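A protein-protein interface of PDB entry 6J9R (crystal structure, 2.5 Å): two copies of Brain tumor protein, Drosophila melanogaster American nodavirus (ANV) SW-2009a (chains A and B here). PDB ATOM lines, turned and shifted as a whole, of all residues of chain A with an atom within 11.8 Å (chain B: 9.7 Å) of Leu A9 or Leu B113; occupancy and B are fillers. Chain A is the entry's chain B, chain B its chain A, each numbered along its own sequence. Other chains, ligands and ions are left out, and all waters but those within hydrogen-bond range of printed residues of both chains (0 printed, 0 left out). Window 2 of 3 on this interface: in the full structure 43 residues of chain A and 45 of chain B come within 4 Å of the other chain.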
ATOM      1  N   ASN A   5       4.094 -14.106 -12.385  1.00  0.00           N
ATOM      2  CA  ASN A   5       4.852 -14.448 -11.184  1.00  0.00           C
ATOM      3  C   ASN A   5       5.716 -13.290 -10.674  1.00  0.00           C
ATOM      4  O   ASN A   5       6.774 -13.501 -10.075  1.00  0.00           O
ATOM      5  CB  ASN A   5       5.730 -15.673 -11.444  1.00  0.00           C
ATOM      6  N   GLU A   6       5.267 -12.066 -10.928  1.00  0.00           N
ATOM      7  CA  GLU A   6       5.852 -10.894 -10.290  1.00  0.00           C
ATOM      8  C   GLU A   6       4.878 -10.409  -9.221  1.00  0.00           C
ATOM      9  O   GLU A   6       5.079  -9.363  -8.598  1.00  0.00           O
ATOM     10  CB  GLU A   6       6.148  -9.789 -11.308  1.00  0.00           C
ATOM     11  N   SER A   7       3.819 -11.189  -9.015  1.00  0.00           N
ATOM     12  CA  SER A   7       2.828 -10.896  -7.988  1.00  0.00           C
ATOM     13  C   SER A   7       3.266 -11.467  -6.643  1.00  0.00           C
ATOM     14  O   SER A   7       2.936 -10.928  -5.588  1.00  0.00           O
ATOM     15  CB  SER A   7       1.461 -11.461  -8.388  1.00  0.00           C
ATOM     16  N   ALA A   8       4.022 -12.556  -6.694  1.00  0.00           N
ATOM     17  CA  ALA A   8       4.662 -13.115  -5.510  1.00  0.00           C
ATOM     18  C   ALA A   8       5.618 -12.105  -4.888  1.00  0.00           C
ATOM     19  O   ALA A   8       5.712 -12.006  -3.667  1.00  0.00           O
ATOM     20  CB  ALA A   8       5.402 -14.398  -5.863  1.00  0.00           C
ATOM     21  N   LEU A   9       6.325 -11.365  -5.739  1.00  0.00           N
ATOM     22  CA  LEU A   9       7.225 -10.308  -5.303  1.00  0.00           C
ATOM     23  C   LEU A   9       6.488  -9.150  -4.626  1.00  0.00           C
ATOM     24  O   LEU A   9       6.898  -8.701  -3.553  1.00  0.00           O
ATOM     25  CB  LEU A   9       8.028  -9.768  -6.491  1.00  0.00           C
ATOM     26  CG  LEU A   9       9.562  -9.797  -6.403  1.00  0.00           C
ATOM     27  CD1 LEU A   9      10.206  -8.921  -7.476  1.00  0.00           C
ATOM     28  CD2 LEU A   9      10.015  -9.391  -4.998  1.00  0.00           C
ATOM     29  N   GLN A  10       5.417  -8.659  -5.248  1.00  0.00           N
ATOM     30  CA  GLN A  10       4.675  -7.534  -4.684  1.00  0.00           C
ATOM     31  C   GLN A  10       4.039  -7.909  -3.357  1.00  0.00           C
ATOM     32  O   GLN A  10       3.945  -7.081  -2.455  1.00  0.00           O
ATOM     33  CB  GLN A  10       3.599  -7.041  -5.653  1.00  0.00           C
ATOM     34  CG  GLN A  10       4.120  -6.161  -6.778  1.00  0.00           C
ATOM     35  N   THR A  11       3.608  -9.161  -3.239  1.00  0.00           N
ATOM     36  CA  THR A  11       3.024  -9.639  -1.993  1.00  0.00           C
ATOM     37  C   THR A  11       4.126  -9.684  -0.936  1.00  0.00           C
ATOM     38  O   THR A  11       3.927  -9.284   0.206  1.00  0.00           O
ATOM     39  CB  THR A  11       2.357 -11.026  -2.153  1.00  0.00           C
ATOM     40  N   LEU A  12       5.299 -10.147  -1.336  1.00  0.00           N
ATOM     41  CA  LEU A  12       6.439 -10.169  -0.440  1.00  0.00           C
ATOM     42  C   LEU A  12       6.785  -8.778   0.056  1.00  0.00           C
ATOM     43  O   LEU A  12       6.948  -8.560   1.259  1.00  0.00           O
ATOM     44  CB  LEU A  12       7.650 -10.764  -1.126  1.00  0.00           C
ATOM     45  CG  LEU A  12       8.863 -10.747  -0.210  1.00  0.00           C
ATOM     46  CD1 LEU A  12       8.582 -11.629   1.007  1.00  0.00           C
ATOM     47  CD2 LEU A  12      10.103 -11.208  -0.963  1.00  0.00           C
ATOM     48  N   LEU A  13       6.898  -7.837  -0.874  1.00  0.00           N
ATOM     49  CA  LEU A  13       7.284  -6.478  -0.525  1.00  0.00           C
ATOM     50  C   LEU A  13       6.273  -5.810   0.397  1.00  0.00           C
ATOM     51  O   LEU A  13       6.644  -5.249   1.427  1.00  0.00           O
ATOM     52  CB  LEU A  13       7.460  -5.635  -1.788  1.00  0.00           C
ATOM     53  CG  LEU A  13       8.595  -6.111  -2.693  1.00  0.00           C
ATOM     54  CD1 LEU A  13       8.574  -5.369  -4.011  1.00  0.00           C
ATOM     55  CD2 LEU A  13       9.948  -5.976  -2.009  1.00  0.00           C
ATOM     56  N   ALA A  14       4.995  -5.902   0.041  1.00  0.00           N
ATOM     57  CA  ALA A  14       3.952  -5.277   0.843  1.00  0.00           C
ATOM     58  C   ALA A  14       3.925  -5.909   2.219  1.00  0.00           C
ATOM     59  O   ALA A  14       3.755  -5.216   3.216  1.00  0.00           O
ATOM     60  CB  ALA A  14       2.579  -5.393   0.163  1.00  0.00           C
ATOM     61  N   ASP A  15       4.130  -7.223   2.264  1.00  0.00           N
ATOM     62  CA  ASP A  15       4.157  -7.950   3.520  1.00  0.00           C
ATOM     63  C   ASP A  15       5.285  -7.449   4.420  1.00  0.00           C
ATOM     64  O   ASP A  15       5.067  -7.196   5.611  1.00  0.00           O
ATOM     65  CB  ASP A  15       4.298  -9.449   3.254  1.00  0.00           C
ATOM     66  CG  ASP A  15       4.423 -10.258   4.530  1.00  0.00           C
ATOM     67  OD1 ASP A  15       3.768  -9.909   5.536  1.00  0.00           O
ATOM     68  OD2 ASP A  15       5.161 -11.263   4.516  1.00  0.00           O
ATOM     69  N   MET A  16       6.478  -7.295   3.845  1.00  0.00           N
ATOM     70  CA  MET A  16       7.615  -6.726   4.560  1.00  0.00           C
ATOM     71  C   MET A  16       7.306  -5.317   5.033  1.00  0.00           C
ATOM     72  O   MET A  16       7.569  -4.975   6.186  1.00  0.00           O
ATOM     73  CB  MET A  16       8.867  -6.693   3.681  1.00  0.00           C
ATOM     74  CG  MET A  16       9.397  -8.042   3.277  1.00  0.00           C
ATOM     75  SD  MET A  16      10.939  -7.856   2.100  1.00  0.00           S
ATOM     76  CE  MET A  16      12.136  -6.916   3.345  1.00  0.00           C
ATOM     77  N   ARG A  17       6.749  -4.500   4.142  1.00  0.00           N
ATOM     78  CA  ARG A  17       6.483  -3.098   4.473  1.00  0.00           C
ATOM     79  C   ARG A  17       5.402  -2.996   5.550  1.00  0.00           C
ATOM     80  O   ARG A  17       5.427  -2.088   6.386  1.00  0.00           O
ATOM     81  CB  ARG A  17       6.081  -2.302   3.226  1.00  0.00           C
ATOM     82  CG  ARG A  17       7.190  -2.239   2.178  1.00  0.00           C
ATOM     83  CD  ARG A  17       6.936  -1.203   1.092  1.00  0.00           C
ATOM     84  NE  ARG A  17       7.724  -0.014   1.404  1.00  0.00           N
ATOM     85  CZ  ARG A  17       8.770   0.400   0.693  1.00  0.00           C
ATOM     86  NH1 ARG A  17       9.119  -0.258  -0.395  1.00  0.00           N
ATOM     87  NH2 ARG A  17       9.456   1.476   1.063  1.00  0.00           N
ATOM     88  N   GLY A  18       4.473  -3.949   5.532  1.00  0.00           N
ATOM     89  CA  GLY A  18       3.426  -4.032   6.535  1.00  0.00           C
ATOM     90  C   GLY A  18       3.977  -4.378   7.899  1.00  0.00           C
ATOM     91  O   GLY A  18       3.612  -3.754   8.901  1.00  0.00           O
ATOM     92  N   THR B  98      16.260  -2.868   1.427  1.00  0.00           N
ATOM     93  CA  THR B  98      16.081  -4.052   0.609  1.00  0.00           C
ATOM     94  C   THR B  98      14.831  -3.930  -0.253  1.00  0.00           C
ATOM     95  O   THR B  98      14.842  -4.352  -1.411  1.00  0.00           O
ATOM     96  CB  THR B  98      16.042  -5.319   1.455  1.00  0.00           C
ATOM     97  OG1 THR B  98      17.294  -5.452   2.150  1.00  0.00           O
ATOM     98  CG2 THR B  98      15.856  -6.527   0.578  1.00  0.00           C
ATOM     99  N   CYS B  99      13.764  -3.360   0.297  1.00  0.00           N
ATOM    100  CA  CYS B  99      12.551  -3.129  -0.483  1.00  0.00           C
ATOM    101  C   CYS B  99      12.809  -2.161  -1.628  1.00  0.00           C
ATOM    102  O   CYS B  99      12.388  -2.384  -2.770  1.00  0.00           O
ATOM    103  CB  CYS B  99      11.433  -2.571   0.389  1.00  0.00           C
ATOM    104  SG  CYS B  99      10.734  -3.752   1.537  1.00  0.00           S
ATOM    105  N   ALA B 101      15.657  -1.483  -2.988  1.00  0.00           N
ATOM    106  CA  ALA B 101      16.553  -2.071  -3.970  1.00  0.00           C
ATOM    107  C   ALA B 101      15.748  -2.974  -4.912  1.00  0.00           C
ATOM    108  O   ALA B 101      15.996  -3.007  -6.111  1.00  0.00           O
ATOM    109  CB  ALA B 101      17.691  -2.839  -3.285  1.00  0.00           C
ATOM    110  N   VAL B 102      14.781  -3.699  -4.365  1.00  0.00           N
ATOM    111  CA  VAL B 102      13.959  -4.605  -5.157  1.00  0.00           C
ATOM    112  C   VAL B 102      13.028  -3.847  -6.092  1.00  0.00           C
ATOM    113  O   VAL B 102      12.909  -4.152  -7.279  1.00  0.00           O
ATOM    114  CB  VAL B 102      13.117  -5.542  -4.262  1.00  0.00           C
ATOM    115  CG1 VAL B 102      11.995  -6.176  -5.078  1.00  0.00           C
ATOM    116  CG2 VAL B 102      14.002  -6.605  -3.620  1.00  0.00           C
ATOM    117  N   GLU B 103      12.385  -2.830  -5.550  1.00  0.00           N
ATOM    118  CA  GLU B 103      11.411  -2.064  -6.314  1.00  0.00           C
ATOM    119  C   GLU B 103      12.016  -1.323  -7.511  1.00  0.00           C
ATOM    120  O   GLU B 103      11.305  -1.008  -8.455  1.00  0.00           O
ATOM    121  CB  GLU B 103      10.710  -1.098  -5.365  1.00  0.00           C
ATOM    122  CG  GLU B 103       9.646  -1.786  -4.540  1.00  0.00           C
ATOM    123  CD  GLU B 103       9.422  -1.118  -3.204  1.00  0.00           C
ATOM    124  OE1 GLU B 103      10.049  -0.064  -2.946  1.00  0.00           O
ATOM    125  OE2 GLU B 103       8.605  -1.639  -2.410  1.00  0.00           O
ATOM    126  N   ARG B 104      13.314  -1.034  -7.463  1.00  0.00           N
ATOM    127  CA  ARG B 104      13.970  -0.309  -8.544  1.00  0.00           C
ATOM    128  C   ARG B 104      14.818  -1.226  -9.424  1.00  0.00           C
ATOM    129  O   ARG B 104      15.378  -0.780 -10.414  1.00  0.00           O
ATOM    130  CB  ARG B 104      14.824   0.830  -8.003  1.00  0.00           C
ATOM    131  CG  ARG B 104      15.956   0.393  -7.167  1.00  0.00           C
ATOM    132  CD  ARG B 104      16.967   1.510  -6.958  1.00  0.00           C
ATOM    133  NE  ARG B 104      18.147   0.947  -6.309  1.00  0.00           N
ATOM    134  CZ  ARG B 104      18.305   0.826  -4.989  1.00  0.00           C
ATOM    135  NH1 ARG B 104      19.402   0.255  -4.505  1.00  0.00           N
ATOM    136  NH2 ARG B 104      17.378   1.271  -4.160  1.00  0.00           N
ATOM    137  N   SER B 105      14.928  -2.498  -9.065  1.00  0.00           N
ATOM    138  CA  SER B 105      15.814  -3.409  -9.797  1.00  0.00           C
ATOM    139  C   SER B 105      15.287  -3.787 -11.182  1.00  0.00           C
ATOM    140  O   SER B 105      14.133  -4.167 -11.340  1.00  0.00           O
ATOM    141  CB  SER B 105      16.060  -4.697  -8.994  1.00  0.00           C
ATOM    142  OG  SER B 105      17.129  -5.449  -9.569  1.00  0.00           O
ATOM    143  N   PRO B 106      16.149  -3.679 -12.191  1.00  0.00           N
ATOM    144  CA  PRO B 106      15.849  -4.161 -13.541  1.00  0.00           C
ATOM    145  C   PRO B 106      15.614  -5.658 -13.518  1.00  0.00           C
ATOM    146  O   PRO B 106      14.784  -6.196 -14.249  1.00  0.00           O
ATOM    147  CB  PRO B 106      17.128  -3.854 -14.328  1.00  0.00           C
ATOM    148  CG  PRO B 106      17.891  -2.882 -13.495  1.00  0.00           C
ATOM    149  CD  PRO B 106      17.524  -3.170 -12.076  1.00  0.00           C
ATOM    150  N   ALA B 107      16.400  -6.318 -12.682  1.00  0.00           N
ATOM    151  CA  ALA B 107      16.365  -7.760 -12.525  1.00  0.00           C
ATOM    152  C   ALA B 107      16.900  -8.139 -11.138  1.00  0.00           C
ATOM    153  O   ALA B 107      18.102  -8.282 -10.974  1.00  0.00           O
ATOM    154  CB  ALA B 107      17.203  -8.418 -13.616  1.00  0.00           C
ATOM    155  N   PRO B 108      16.014  -8.335 -10.152  1.00  0.00           N
ATOM    156  CA  PRO B 108      16.500  -8.609  -8.784  1.00  0.00           C
ATOM    157  C   PRO B 108      17.442  -9.819  -8.700  1.00  0.00           C
ATOM    158  O   PRO B 108      17.022 -10.923  -8.986  1.00  0.00           O
ATOM    159  CB  PRO B 108      15.201  -8.871  -7.995  1.00  0.00           C
ATOM    160  CG  PRO B 108      14.116  -8.179  -8.802  1.00  0.00           C
ATOM    161  CD  PRO B 108      14.543  -8.287 -10.242  1.00  0.00           C
ATOM    162  N   PRO B 109      18.700  -9.611  -8.290  1.00  0.00           N
ATOM    163  CA  PRO B 109      19.632 -10.741  -8.127  1.00  0.00           C
ATOM    164  C   PRO B 109      19.099 -11.704  -7.084  1.00  0.00           C
ATOM    165  O   PRO B 109      18.346 -11.306  -6.167  1.00  0.00           O
ATOM    166  CB  PRO B 109      20.940 -10.080  -7.622  1.00  0.00           C
ATOM    167  CG  PRO B 109      20.787  -8.628  -7.915  1.00  0.00           C
ATOM    168  CD  PRO B 109      19.299  -8.328  -7.889  1.00  0.00           C
ATOM    169  N   SER B 110      19.539 -12.947  -7.169  1.00  0.00           N
ATOM    170  CA  SER B 110      19.084 -13.956  -6.231  1.00  0.00           C
ATOM    171  C   SER B 110      19.478 -13.637  -4.783  1.00  0.00           C
ATOM    172  O   SER B 110      18.777 -14.028  -3.836  1.00  0.00           O
ATOM    173  CB  SER B 110      19.640 -15.313  -6.630  1.00  0.00           C
ATOM    174  OG  SER B 110      21.049 -15.306  -6.570  1.00  0.00           O
ATOM    175  N   SER B 111      20.593 -12.934  -4.606  1.00  0.00           N
ATOM    176  CA  SER B 111      21.054 -12.600  -3.261  1.00  0.00           C
ATOM    177  C   SER B 111      20.132 -11.545  -2.635  1.00  0.00           C
ATOM    178  O   SER B 111      19.842 -11.573  -1.440  1.00  0.00           O
ATOM    179  CB  SER B 111      22.493 -12.121  -3.306  1.00  0.00           C
ATOM    180  OG  SER B 111      22.589 -10.879  -3.969  1.00  0.00           O
ATOM    181  N   LEU B 112      19.661 -10.620  -3.461  1.00  0.00           N
ATOM    182  CA  LEU B 112      18.741  -9.600  -2.995  1.00  0.00           C
ATOM    183  C   LEU B 112      17.398 -10.245  -2.626  1.00  0.00           C
ATOM    184  O   LEU B 112      16.760  -9.879  -1.638  1.00  0.00           O
ATOM    185  CB  LEU B 112      18.548  -8.528  -4.063  1.00  0.00           C
ATOM    186  CG  LEU B 112      17.630  -7.394  -3.643  1.00  0.00           C
ATOM    187  CD1 LEU B 112      18.271  -6.713  -2.421  1.00  0.00           C
ATOM    188  CD2 LEU B 112      17.424  -6.415  -4.778  1.00  0.00           C
ATOM    189  N   LEU B 113      16.957 -11.207  -3.421  1.00  0.00           N
ATOM    190  CA  LEU B 113      15.695 -11.866  -3.106  1.00  0.00           C
ATOM    191  C   LEU B 113      15.848 -12.708  -1.857  1.00  0.00           C
ATOM    192  O   LEU B 113      14.925 -12.793  -1.058  1.00  0.00           O
ATOM    193  CB  LEU B 113      15.207 -12.723  -4.281  1.00  0.00           C
ATOM    194  CG  LEU B 113      14.799 -11.948  -5.541  1.00  0.00           C
ATOM    195  CD1 LEU B 113      14.583 -12.890  -6.720  1.00  0.00           C
ATOM    196  CD2 LEU B 113      13.561 -11.082  -5.313  1.00  0.00           C
ATOM    197  N   THR B 114      17.023 -13.303  -1.671  1.00  0.00           N
ATOM    198  CA  THR B 114      17.275 -14.102  -0.477  1.00  0.00           C
ATOM    199  C   THR B 114      17.254 -13.234   0.783  1.00  0.00           C
ATOM    200  O   THR B 114      16.646 -13.587   1.818  1.00  0.00           O
ATOM    201  CB  THR B 114      18.624 -14.796  -0.570  1.00  0.00           C
ATOM    202  OG1 THR B 114      18.597 -15.740  -1.645  1.00  0.00           O
ATOM    203  CG2 THR B 114      18.946 -15.518   0.719  1.00  0.00           C
ATOM    204  N   GLU B 115      17.886 -12.075   0.646  1.00  0.00           N
ATOM    205  CA  GLU B 115      17.965 -11.070   1.692  1.00  0.00           C
ATOM    206  C   GLU B 115      16.580 -10.583   2.064  1.00  0.00           C
ATOM    207  O   GLU B 115      16.277 -10.451   3.253  1.00  0.00           O
ATOM    208  CB  GLU B 115      18.829  -9.900   1.219  1.00  0.00           C
ATOM    209  CG  GLU B 115      19.111  -8.855   2.262  1.00  0.00           C
ATOM    210  CD  GLU B 115      19.942  -9.407   3.447  1.00  0.00           C
ATOM    211  OE1 GLU B 115      20.589 -10.478   3.325  1.00  0.00           O
ATOM    212  OE2 GLU B 115      19.997  -8.735   4.493  1.00  0.00           O
ATOM    213  N   ALA B 116      15.733 -10.326   1.056  1.00  0.00           N
ATOM    214  CA  ALA B 116      14.357  -9.932   1.347  1.00  0.00           C
ATOM    215  C   ALA B 116      13.657 -11.017   2.176  1.00  0.00           C
ATOM    216  O   ALA B 116      13.043 -10.718   3.189  1.00  0.00           O
ATOM    217  CB  ALA B 116      13.566  -9.654   0.046  1.00  0.00           C
ATOM    218  N   LEU B 117      13.802 -12.275   1.774  1.00  0.00           N
ATOM    219  CA  LEU B 117      13.174 -13.377   2.485  1.00  0.00           C
ATOM    220  C   LEU B 117      13.644 -13.529   3.937  1.00  0.00           C
ATOM    221  O   LEU B 117      12.845 -13.790   4.844  1.00  0.00           O
ATOM    222  CB  LEU B 117      13.451 -14.675   1.744  1.00  0.00           C
ATOM    223  CG  LEU B 117      12.417 -15.258   0.780  1.00  0.00           C
ATOM    224  CD1 LEU B 117      11.327 -14.278   0.418  1.00  0.00           C
ATOM    225  CD2 LEU B 117      13.128 -15.739  -0.442  1.00  0.00           C
ATOM    226  N   LEU B 118      14.945 -13.381   4.145  1.00  0.00           N
ATOM    227  CA  LEU B 118      15.521 -13.475   5.474  1.00  0.00           C
ATOM    228  C   LEU B 118      15.045 -12.325   6.354  1.00  0.00           C
ATOM    229  O   LEU B 118      14.663 -12.522   7.514  1.00  0.00           O
ATOM    230  CB  LEU B 118      17.046 -13.491   5.379  1.00  0.00           C
ATOM    231  CG  LEU B 118      17.562 -14.831   4.850  1.00  0.00           C
ATOM    232  CD1 LEU B 118      19.064 -14.822   4.643  1.00  0.00           C
ATOM    233  CD2 LEU B 118      17.158 -15.929   5.843  1.00  0.00           C
ATOM    234  N   LEU B 119      15.052 -11.126   5.789  1.00  0.00           N
ATOM    235  CA  LEU B 119      14.645  -9.952   6.533  1.00  0.00           C
ATOM    236  C   LEU B 119      13.159 -10.050   6.858  1.00  0.00           C
ATOM    237  O   LEU B 119      12.713  -9.611   7.932  1.00  0.00           O
ATOM    238  CB  LEU B 119      14.971  -8.688   5.743  1.00  0.00           C
ATOM    239  CG  LEU B 119      16.467  -8.320   5.752  1.00  0.00           C
ATOM    240  CD1 LEU B 119      16.716  -7.135   4.840  1.00  0.00           C
ATOM    241  CD2 LEU B 119      16.995  -8.041   7.153  1.00  0.00           C
ATOM    242  N   ARG B 120      12.383 -10.626   5.940  1.00  0.00           N
ATOM    243  CA  ARG B 120      10.949 -10.735   6.188  1.00  0.00           C
ATOM    244  C   ARG B 120      10.733 -11.634   7.388  1.00  0.00           C
ATOM    245  O   ARG B 120       9.913 -11.338   8.237  1.00  0.00           O
ATOM    246  CB  ARG B 120      10.190 -11.284   4.985  1.00  0.00           C
ATOM    247  CG  ARG B 120       8.661 -11.307   5.191  1.00  0.00           C
ATOM    248  CD  ARG B 120       8.088 -12.666   5.576  1.00  0.00           C
ATOM    249  NE  ARG B 120       7.663 -13.429   4.410  1.00  0.00           N
ATOM    250  CZ  ARG B 120       8.399 -14.384   3.845  1.00  0.00           C
ATOM    251  NH1 ARG B 120       7.932 -15.029   2.777  1.00  0.00           N
ATOM    252  NH2 ARG B 120       9.604 -14.694   4.348  1.00  0.00           N
ATOM    253  N   LYS B 121      11.502 -12.718   7.460  1.00  0.00           N
ATOM    254  CA  LYS B 121      11.404 -13.650   8.578  1.00  0.00           C
ATOM    255  C   LYS B 121      11.782 -12.967   9.895  1.00  0.00           C
ATOM    256  O   LYS B 121      11.051 -13.064  10.883  1.00  0.00           O
ATOM    257  CB  LYS B 121      12.296 -14.867   8.331  1.00  0.00           C
ATOM    258  CG  LYS B 121      12.209 -15.944   9.400  1.00  0.00           C
ATOM    259  CD  LYS B 121      11.227 -17.033   9.004  1.00  0.00           C
ATOM    260  CE  LYS B 121      11.153 -18.138  10.052  1.00  0.00           C
ATOM    261  NZ  LYS B 121      12.483 -18.401  10.674  1.00  0.00           N
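The guanidinium group (NE) of Arg B120 lies within salt-bridge range of the side-chain carboxylate (OD2) of Asp A15 (3.3 Å).
The side-chain sulfur of Met A16 sits close to the backbone carbonyl oxygen of Ala B116, 3.7 Å away.
The guanidinium group (NH1) of Arg A17 lies within salt-bridge range of the side-chain carboxylate (OE2) of Glu B103.
O of Leu B117 lies within hydrogen-bond range of NH2 of Arg B120 (3.4 Å).
Leu A9 touches Val B102 (CD2 to CG1, 3.8 Å).
Leu A9 touches Leu B113.
Leu A12 touches Ala B116.
CD1 of Leu B117 touches CD2 of Leu A12, 3.6 Å away.
CD1 of Leu A12 touches NH1 of Arg B120, 3.9 Å away.
Leu A13 touches Val B102.
Glu B103 touches Leu A13.
Cys B99 touches Met A16 (SG to CE, 3.9 Å).
Met A16 touches Arg B120 (CG to CB, 3.7 Å).
Arg A17 touches Cys B99 (NH1 to CB, 3.4 Å).
No residue of chain B comes within 4 Å of Ala A8.
No residue of chain B comes within 4 Å of Gln A10.
Printed residues of chain B within 4 Å of Asp A15: Arg B120 (3.3 Å).
Printed residues of chain B within 4 Å of Met A16: Cys B99, Ala B116 and Arg B120.
Of the printed residues of chain A, Cys B99 touches Met A16 and Arg A17.
No residue of chain A comes within 4 Å of Pro B108.
No residue of chain A comes within 4 Å of Ser B110.
Ser B111 touches none of the printed residues of chain A.
Of chain A, only Leu A9 comes within 4 Å of Leu B113.
Thr B114 touches none of the printed residues of chain A.
Of chain A, only Leu A12 and Met A16 come within 4 Å of Ala B116.
Leu B117 touches just one residue of chain A: Leu A12.
Of the printed residues of chain A, Arg B120 touches Leu A12, Asp A15 and Met A16.
The nearest residue of chain B that does not touch Leu A9 is Pro B108 (4.2 Å).
Of the 23 printed residues of chain B, 7 touch a printed residue of chain A.
Along chain B the printed residues that touch a printed residue of chain A span positions 99 to 120.
Printed residues of chain A that touch a printed residue of chain B: Leu A9, Leu A12, Leu A13, Asp A15, Met A16 and Arg A17.
Hydrophobic or aromatic side chains of chain A within 4 Å of the printed part of chain B: Leu A9, Leu A12, Leu A13 and Met A16.
Along chain A the printed residues that touch a printed residue of chain B span positions 9 to 17.
Among the printed residues, 13 pairs touch across the chains.
Among the printed residues, Asp or Glu carboxylates within 4 Å of a Lys or Arg side-chain nitrogen of the other chain: Asp A15 with Arg B120 and Arg A17 with Glu B103.
No position is printed for both chains.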
